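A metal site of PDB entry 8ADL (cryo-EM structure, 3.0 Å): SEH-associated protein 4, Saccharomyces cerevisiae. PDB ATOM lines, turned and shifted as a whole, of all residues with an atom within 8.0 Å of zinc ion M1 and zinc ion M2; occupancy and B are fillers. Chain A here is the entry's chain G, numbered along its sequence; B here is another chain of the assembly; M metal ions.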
ATOM      1  N   SER A1003      -6.965   8.382  -9.901  1.00  0.00           N
ATOM      2  CA  SER A1003      -6.631   7.867  -8.580  1.00  0.00           C
ATOM      3  C   SER A1003      -7.046   8.911  -7.558  1.00  0.00           C
ATOM      4  O   SER A1003      -6.253   9.742  -7.109  1.00  0.00           O
ATOM      5  CB  SER A1003      -5.149   7.523  -8.484  1.00  0.00           C
ATOM      6  OG  SER A1003      -4.751   7.390  -7.123  1.00  0.00           O
ATOM      7  N   PHE A1004      -8.327   8.884  -7.186  1.00  0.00           N
ATOM      8  CA  PHE A1004      -8.878   9.857  -6.257  1.00  0.00           C
ATOM      9  C   PHE A1004      -8.453   9.535  -4.838  1.00  0.00           C
ATOM     10  O   PHE A1004      -8.712   8.431  -4.339  1.00  0.00           O
ATOM     11  CB  PHE A1004     -10.399   9.886  -6.356  1.00  0.00           C
ATOM     12  CG  PHE A1004     -10.932  10.907  -7.323  1.00  0.00           C
ATOM     13  CD1 PHE A1004     -10.957  12.241  -6.980  1.00  0.00           C
ATOM     14  CD2 PHE A1004     -11.412  10.522  -8.560  1.00  0.00           C
ATOM     15  CE1 PHE A1004     -11.461  13.183  -7.861  1.00  0.00           C
ATOM     16  CE2 PHE A1004     -11.911  11.451  -9.440  1.00  0.00           C
ATOM     17  CZ  PHE A1004     -11.933  12.793  -9.093  1.00  0.00           C
ATOM     18  N   CYS A1005      -7.823  10.489  -4.176  1.00  0.00           N
ATOM     19  CA  CYS A1005      -7.566  10.359  -2.747  1.00  0.00           C
ATOM     20  C   CYS A1005      -8.856  10.552  -1.983  1.00  0.00           C
ATOM     21  O   CYS A1005      -9.695  11.388  -2.346  1.00  0.00           O
ATOM     22  CB  CYS A1005      -6.516  11.371  -2.289  1.00  0.00           C
ATOM     23  SG  CYS A1005      -6.192  11.318  -0.516  1.00  0.00           S
ATOM     24  N   LEU A1006      -9.025   9.787  -0.910  1.00  0.00           N
ATOM     25  CA  LEU A1006     -10.233   9.857  -0.092  1.00  0.00           C
ATOM     26  C   LEU A1006     -10.086  10.821   1.083  1.00  0.00           C
ATOM     27  O   LEU A1006     -11.008  10.914   1.896  1.00  0.00           O
ATOM     28  CB  LEU A1006     -10.593   8.461   0.412  1.00  0.00           C
ATOM     29  CG  LEU A1006     -10.593   7.395  -0.689  1.00  0.00           C
ATOM     30  CD1 LEU A1006     -10.843   6.020  -0.114  1.00  0.00           C
ATOM     31  CD2 LEU A1006     -11.625   7.732  -1.739  1.00  0.00           C
ATOM     32  N   SER A1007      -8.964  11.528   1.182  1.00  0.00           N
ATOM     33  CA  SER A1007      -8.745  12.523   2.224  1.00  0.00           C
ATOM     34  C   SER A1007      -8.812  13.952   1.699  1.00  0.00           C
ATOM     35  O   SER A1007      -9.478  14.801   2.314  1.00  0.00           O
ATOM     36  CB  SER A1007      -7.401  12.275   2.907  1.00  0.00           C
ATOM     37  OG  SER A1007      -7.367  11.019   3.539  1.00  0.00           O
ATOM     38  N   CYS A1008      -8.149  14.246   0.586  1.00  0.00           N
ATOM     39  CA  CYS A1008      -8.152  15.580   0.012  1.00  0.00           C
ATOM     40  C   CYS A1008      -9.050  15.717  -1.213  1.00  0.00           C
ATOM     41  O   CYS A1008      -9.248  16.839  -1.683  1.00  0.00           O
ATOM     42  CB  CYS A1008      -6.730  16.009  -0.356  1.00  0.00           C
ATOM     43  SG  CYS A1008      -5.889  14.894  -1.500  1.00  0.00           S
ATOM     44  N   ASN A1009      -9.577  14.596  -1.734  1.00  0.00           N
ATOM     45  CA  ASN A1009     -10.524  14.563  -2.855  1.00  0.00           C
ATOM     46  C   ASN A1009      -9.966  15.228  -4.114  1.00  0.00           C
ATOM     47  O   ASN A1009     -10.681  15.925  -4.835  1.00  0.00           O
ATOM     48  CB  ASN A1009     -11.864  15.189  -2.455  1.00  0.00           C
ATOM     49  CG  ASN A1009     -12.525  14.455  -1.312  1.00  0.00           C
ATOM     50  OD1 ASN A1009     -12.173  13.319  -0.995  1.00  0.00           O
ATOM     51  ND2 ASN A1009     -13.479  15.114  -0.669  1.00  0.00           N
ATOM     52  N   HIS A1010      -8.687  15.019  -4.385  1.00  0.00           N
ATOM     53  CA  HIS A1010      -8.038  15.528  -5.593  1.00  0.00           C
ATOM     54  C   HIS A1010      -7.599  14.354  -6.466  1.00  0.00           C
ATOM     55  O   HIS A1010      -6.954  13.422  -5.983  1.00  0.00           O
ATOM     56  CB  HIS A1010      -6.850  16.416  -5.234  1.00  0.00           C
ATOM     57  CG  HIS A1010      -7.215  17.606  -4.414  1.00  0.00           C
ATOM     58  ND1 HIS A1010      -6.485  18.017  -3.318  1.00  0.00           N
ATOM     59  CD2 HIS A1010      -8.238  18.485  -4.524  1.00  0.00           C
ATOM     60  CE1 HIS A1010      -7.039  19.094  -2.794  1.00  0.00           C
ATOM     61  NE2 HIS A1010      -8.111  19.388  -3.502  1.00  0.00           N
ATOM     62  N   GLY A1011      -7.945  14.417  -7.747  1.00  0.00           N
ATOM     63  CA  GLY A1011      -7.757  13.300  -8.659  1.00  0.00           C
ATOM     64  C   GLY A1011      -6.735  13.587  -9.750  1.00  0.00           C
ATOM     65  O   GLY A1011      -6.690  14.681 -10.314  1.00  0.00           O
ATOM     66  N   PHE A1021       4.122  10.991  -7.883  1.00  0.00           N
ATOM     67  CA  PHE A1021       4.334  10.531  -6.518  1.00  0.00           C
ATOM     68  C   PHE A1021       5.573   9.651  -6.372  1.00  0.00           C
ATOM     69  O   PHE A1021       5.916   9.289  -5.246  1.00  0.00           O
ATOM     70  CB  PHE A1021       3.109   9.774  -6.022  1.00  0.00           C
ATOM     71  CG  PHE A1021       2.000  10.669  -5.547  1.00  0.00           C
ATOM     72  CD1 PHE A1021       2.206  11.538  -4.492  1.00  0.00           C
ATOM     73  CD2 PHE A1021       0.767  10.662  -6.171  1.00  0.00           C
ATOM     74  CE1 PHE A1021       1.197  12.370  -4.054  1.00  0.00           C
ATOM     75  CE2 PHE A1021      -0.249  11.498  -5.738  1.00  0.00           C
ATOM     76  CZ  PHE A1021      -0.038  12.354  -4.682  1.00  0.00           C
ATOM     77  N   VAL A1026       3.594  15.008  -1.840  1.00  0.00           N
ATOM     78  CA  VAL A1026       2.546  15.939  -1.477  1.00  0.00           C
ATOM     79  C   VAL A1026       1.530  15.991  -2.624  1.00  0.00           C
ATOM     80  O   VAL A1026       1.831  15.617  -3.754  1.00  0.00           O
ATOM     81  CB  VAL A1026       3.119  17.356  -1.167  1.00  0.00           C
ATOM     82  CG1 VAL A1026       3.497  18.100  -2.454  1.00  0.00           C
ATOM     83  CG2 VAL A1026       2.185  18.171  -0.281  1.00  0.00           C
ATOM     84  N   CYS A1027       0.309  16.390  -2.284  1.00  0.00           N
ATOM     85  CA  CYS A1027      -0.751  16.523  -3.288  1.00  0.00           C
ATOM     86  C   CYS A1027      -0.391  17.634  -4.260  1.00  0.00           C
ATOM     87  O   CYS A1027      -0.021  18.736  -3.838  1.00  0.00           O
ATOM     88  CB  CYS A1027      -2.087  16.818  -2.604  1.00  0.00           C
ATOM     89  SG  CYS A1027      -3.496  16.929  -3.722  1.00  0.00           S
ATOM     90  N   PRO A1028      -0.489  17.395  -5.577  1.00  0.00           N
ATOM     91  CA  PRO A1028      -0.032  18.393  -6.548  1.00  0.00           C
ATOM     92  C   PRO A1028      -0.945  19.604  -6.684  1.00  0.00           C
ATOM     93  O   PRO A1028      -0.532  20.587  -7.322  1.00  0.00           O
ATOM     94  CB  PRO A1028       0.024  17.597  -7.856  1.00  0.00           C
ATOM     95  CG  PRO A1028      -1.039  16.597  -7.682  1.00  0.00           C
ATOM     96  CD  PRO A1028      -0.969  16.171  -6.243  1.00  0.00           C
ATOM     97  N   THR A1029      -2.148  19.566  -6.128  1.00  0.00           N
ATOM     98  CA  THR A1029      -3.077  20.680  -6.261  1.00  0.00           C
ATOM     99  C   THR A1029      -2.611  21.882  -5.439  1.00  0.00           C
ATOM    100  O   THR A1029      -1.996  21.730  -4.378  1.00  0.00           O
ATOM    101  CB  THR A1029      -4.479  20.259  -5.821  1.00  0.00           C
ATOM    102  OG1 THR A1029      -4.436  19.759  -4.477  1.00  0.00           O
ATOM    103  CG2 THR A1029      -5.007  19.180  -6.760  1.00  0.00           C
ATOM    104  N   PRO A1030      -2.901  23.105  -5.909  1.00  0.00           N
ATOM    105  CA  PRO A1030      -2.373  24.303  -5.235  1.00  0.00           C
ATOM    106  C   PRO A1030      -3.081  24.623  -3.918  1.00  0.00           C
ATOM    107  O   PRO A1030      -4.042  25.409  -3.904  1.00  0.00           O
ATOM    108  CB  PRO A1030      -2.580  25.418  -6.263  1.00  0.00           C
ATOM    109  CG  PRO A1030      -3.676  24.920  -7.143  1.00  0.00           C
ATOM    110  CD  PRO A1030      -3.481  23.437  -7.217  1.00  0.00           C
ATOM    111  N   GLY A1031      -2.639  24.015  -2.821  1.00  0.00           N
ATOM    112  CA  GLY A1031      -3.173  24.358  -1.522  1.00  0.00           C
ATOM    113  C   GLY A1031      -3.588  23.172  -0.681  1.00  0.00           C
ATOM    114  O   GLY A1031      -4.375  23.301   0.256  1.00  0.00           O
ATOM    115  N   CYS A1032      -3.054  22.000  -1.006  1.00  0.00           N
ATOM    116  CA  CYS A1032      -3.326  20.770  -0.267  1.00  0.00           C
ATOM    117  C   CYS A1032      -2.042  20.237   0.335  1.00  0.00           C
ATOM    118  O   CYS A1032      -0.994  20.194  -0.332  1.00  0.00           O
ATOM    119  CB  CYS A1032      -3.961  19.713  -1.172  1.00  0.00           C
ATOM    120  SG  CYS A1032      -4.596  18.284  -0.270  1.00  0.00           S
ATOM    121  N   THR A1033      -2.108  19.823   1.595  1.00  0.00           N
ATOM    122  CA  THR A1033      -1.013  19.161   2.285  1.00  0.00           C
ATOM    123  C   THR A1033      -1.511  17.786   2.716  1.00  0.00           C
ATOM    124  O   THR A1033      -1.988  17.599   3.841  1.00  0.00           O
ATOM    125  CB  THR A1033      -0.524  19.974   3.487  1.00  0.00           C
ATOM    126  OG1 THR A1033      -0.472  21.360   3.120  1.00  0.00           O
ATOM    127  CG2 THR A1033       0.860  19.518   3.914  1.00  0.00           C
ATOM    128  N   CYS A1034      -1.415  16.815   1.801  1.00  0.00           N
ATOM    129  CA  CYS A1034      -1.923  15.472   2.044  1.00  0.00           C
ATOM    130  C   CYS A1034      -1.008  14.495   1.303  1.00  0.00           C
ATOM    131  O   CYS A1034      -1.015  14.469   0.062  1.00  0.00           O
ATOM    132  CB  CYS A1034      -3.370  15.327   1.591  1.00  0.00           C
ATOM    133  SG  CYS A1034      -4.013  13.639   1.622  1.00  0.00           S
ATOM    134  N   GLN A1035      -0.255  13.701   2.045  1.00  0.00           N
ATOM    135  CA  GLN A1035       0.653  12.714   1.456  1.00  0.00           C
ATOM    136  C   GLN A1035      -0.171  11.513   1.024  1.00  0.00           C
ATOM    137  O   GLN A1035      -0.427  10.599   1.799  1.00  0.00           O
ATOM    138  CB  GLN A1035       1.739  12.324   2.446  1.00  0.00           C
ATOM    139  CG  GLN A1035       2.290  13.490   3.252  1.00  0.00           C
ATOM    140  CD  GLN A1035       3.542  13.122   4.028  1.00  0.00           C
ATOM    141  OE1 GLN A1035       4.002  11.978   3.981  1.00  0.00           O
ATOM    142  NE2 GLN A1035       4.103  14.092   4.742  1.00  0.00           N
ATOM    143  N   CYS A1036      -0.583  11.519  -0.247  1.00  0.00           N
ATOM    144  CA  CYS A1036      -1.433  10.467  -0.772  1.00  0.00           C
ATOM    145  C   CYS A1036      -0.681   9.182  -1.112  1.00  0.00           C
ATOM    146  O   CYS A1036      -1.334   8.164  -1.394  1.00  0.00           O
ATOM    147  CB  CYS A1036      -2.166  10.958  -2.025  1.00  0.00           C
ATOM    148  SG  CYS A1036      -2.895  12.601  -1.872  1.00  0.00           S
ATOM    149  N   ASN A1037       0.638   9.194  -1.095  1.00  0.00           N
ATOM    150  CA  ASN A1037       1.408   7.995  -1.411  1.00  0.00           C
ATOM    151  C   ASN A1037       2.581   7.843  -0.450  1.00  0.00           C
ATOM    152  O   ASN A1037       2.446   7.268   0.631  1.00  0.00           O
ATOM    153  CB  ASN A1037       1.888   8.036  -2.863  1.00  0.00           C
ATOM    154  CG  ASN A1037       2.394   6.689  -3.360  1.00  0.00           C
ATOM    155  OD1 ASN A1037       2.361   5.691  -2.642  1.00  0.00           O
ATOM    156  ND2 ASN A1037       2.859   6.662  -4.600  1.00  0.00           N
ATOM    157  N   LYS B1051       3.300  24.840  -6.927  1.00  0.00           N
ATOM    158  CA  LYS B1051       3.180  24.416  -5.542  1.00  0.00           C
ATOM    159  C   LYS B1051       4.058  25.266  -4.629  1.00  0.00           C
ATOM    160  O   LYS B1051       3.641  25.622  -3.522  1.00  0.00           O
ATOM    161  CB  LYS B1051       3.532  22.940  -5.415  1.00  0.00           C
ATOM    162  CG  LYS B1051       3.242  22.340  -4.044  1.00  0.00           C
ATOM    163  CD  LYS B1051       1.937  21.552  -4.065  1.00  0.00           C
ATOM    164  CE  LYS B1051       1.286  21.565  -2.692  1.00  0.00           C
ATOM    165  NZ  LYS B1051      -0.065  20.935  -2.713  1.00  0.00           N
ATOM    166  N   TYR B1075      -9.854  21.986  -9.496  1.00  0.00           N
ATOM    167  CA  TYR B1075      -9.650  20.665  -8.909  1.00  0.00           C
ATOM    168  C   TYR B1075     -10.573  20.474  -7.711  1.00  0.00           C
ATOM    169  O   TYR B1075     -10.162  20.035  -6.627  1.00  0.00           O
ATOM    170  CB  TYR B1075      -8.193  20.474  -8.489  1.00  0.00           C
ATOM    171  CG  TYR B1075      -7.193  21.046  -9.476  1.00  0.00           C
ATOM    172  CD1 TYR B1075      -6.918  20.402 -10.667  1.00  0.00           C
ATOM    173  CD2 TYR B1075      -6.532  22.243  -9.197  1.00  0.00           C
ATOM    174  CE1 TYR B1075      -6.001  20.920 -11.564  1.00  0.00           C
ATOM    175  CE2 TYR B1075      -5.615  22.760 -10.093  1.00  0.00           C
ATOM    176  CZ  TYR B1075      -5.355  22.104 -11.274  1.00  0.00           C
ATOM    177  OH  TYR B1075      -4.444  22.619 -12.162  1.00  0.00           O
ATOM    178  N   THR B1106      -7.347   4.795   2.672  1.00  0.00           N
ATOM    179  CA  THR B1106      -7.534   6.190   3.065  1.00  0.00           C
ATOM    180  C   THR B1106      -6.930   7.194   2.100  1.00  0.00           C
ATOM    181  O   THR B1106      -7.352   8.359   2.131  1.00  0.00           O
ATOM    182  CB  THR B1106      -6.951   6.433   4.462  1.00  0.00           C
ATOM    183  OG1 THR B1106      -7.120   7.809   4.813  1.00  0.00           O
ATOM    184  CG2 THR B1106      -5.473   6.068   4.509  1.00  0.00           C
ATOM    185  N   ARG B1107      -5.986   6.800   1.246  1.00  0.00           N
ATOM    186  CA  ARG B1107      -5.359   7.715   0.293  1.00  0.00           C
ATOM    187  C   ARG B1107      -5.124   6.990  -1.020  1.00  0.00           C
ATOM    188  O   ARG B1107      -4.760   5.811  -1.036  1.00  0.00           O
ATOM    189  CB  ARG B1107      -4.026   8.245   0.848  1.00  0.00           C
ATOM    190  CG  ARG B1107      -4.175   9.297   1.938  1.00  0.00           C
ATOM    191  CD  ARG B1107      -3.132   9.120   3.024  1.00  0.00           C
ATOM    192  NE  ARG B1107      -3.243  10.157   4.049  1.00  0.00           N
ATOM    193  CZ  ARG B1107      -2.359  10.356   5.010  1.00  0.00           C
ATOM    194  NH1 ARG B1107      -1.273   9.601   5.110  1.00  0.00           N
ATOM    195  NH2 ARG B1107      -2.554  11.330   5.895  1.00  0.00           N
ATOM    196  N   SER B1108      -5.344   7.718  -2.125  1.00  0.00           N
ATOM    197  CA  SER B1108      -5.016   7.294  -3.484  1.00  0.00           C
ATOM    198  C   SER B1108      -5.733   5.988  -3.865  1.00  0.00           C
ATOM    199  O   SER B1108      -5.131   4.938  -4.075  1.00  0.00           O
ATOM    200  CB  SER B1108      -3.495   7.145  -3.668  1.00  0.00           C
ATOM    201  OG  SER B1108      -3.147   7.057  -5.036  1.00  0.00           O
HETATM  202 ZN    ZN M   1      -4.720  13.126  -0.534  1.00  0.00          ZN
HETATM  203 ZN    ZN M   2      -5.158  17.002  -2.115  1.00  0.00          ZN
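The side-chain amino group of Lys 1051 of chain B sits at hydrogen-bond distance from the backbone carbonyl oxygen of Cys 1027 (2.5 Å). N of Ser 1007 lies close to SG of Cys 1005 (3.3 Å). OG1 of Thr 1029 sits close to SG of Cys 1027, 3.1 Å away. The backbone carbonyl oxygen (O) of Cys 1005 lies close to the side-chain amide oxygen (OD1) of Asn 1009 (3.4 Å). The backbone carbonyl oxygen (O) of Cys 1034 sits at hydrogen-bond distance from the backbone NH (N) of Cys 1027. O of Thr 1029 sits at hydrogen-bond distance from NZ of Lys 1051 of chain B (2.7 Å). ND1 of His 1010 lies close to OG1 of Thr 1029. O of Cys 1032 lies within hydrogen-bond range of NZ of Lys 1051 of chain B, 2.7 Å away.
Within 4 Å of zinc ion M1: Cys 1005, Cys 1008, Cys 1034 and Cys 1036.
OG1 of Thr 1029 touches zinc ion M2, at 3.7 Å. Of the 27 residues printed, 5 come within 4 Å of zinc ion M2. The nearest printed residue that does not touch zinc ion M2 is Cys 1034 (4.4 Å).
Zinc ion M1 is bound by the side-chain sulfur (SG) of Cys 1036 (2.3 Å), the side-chain sulfur (SG) of Cys 1034 (2.3 Å), the side-chain sulfur (SG) of Cys 1008 (2.3 Å) and the side-chain sulfur (SG) of Cys 1005 (2.3 Å).
Zinc ion M2 is bound by ND1 of His 1010 (2.1 Å). SG of Cys 1027 binds zinc ion M2, at 2.3 Å. Zinc ion M2 is bound by SG of Cys 1008 (2.3 Å). The side-chain sulfur (SG) of Cys 1032 binds zinc ion M2, 2.3 Å away. Zinc ion M2 has four donor atoms within binding distance.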
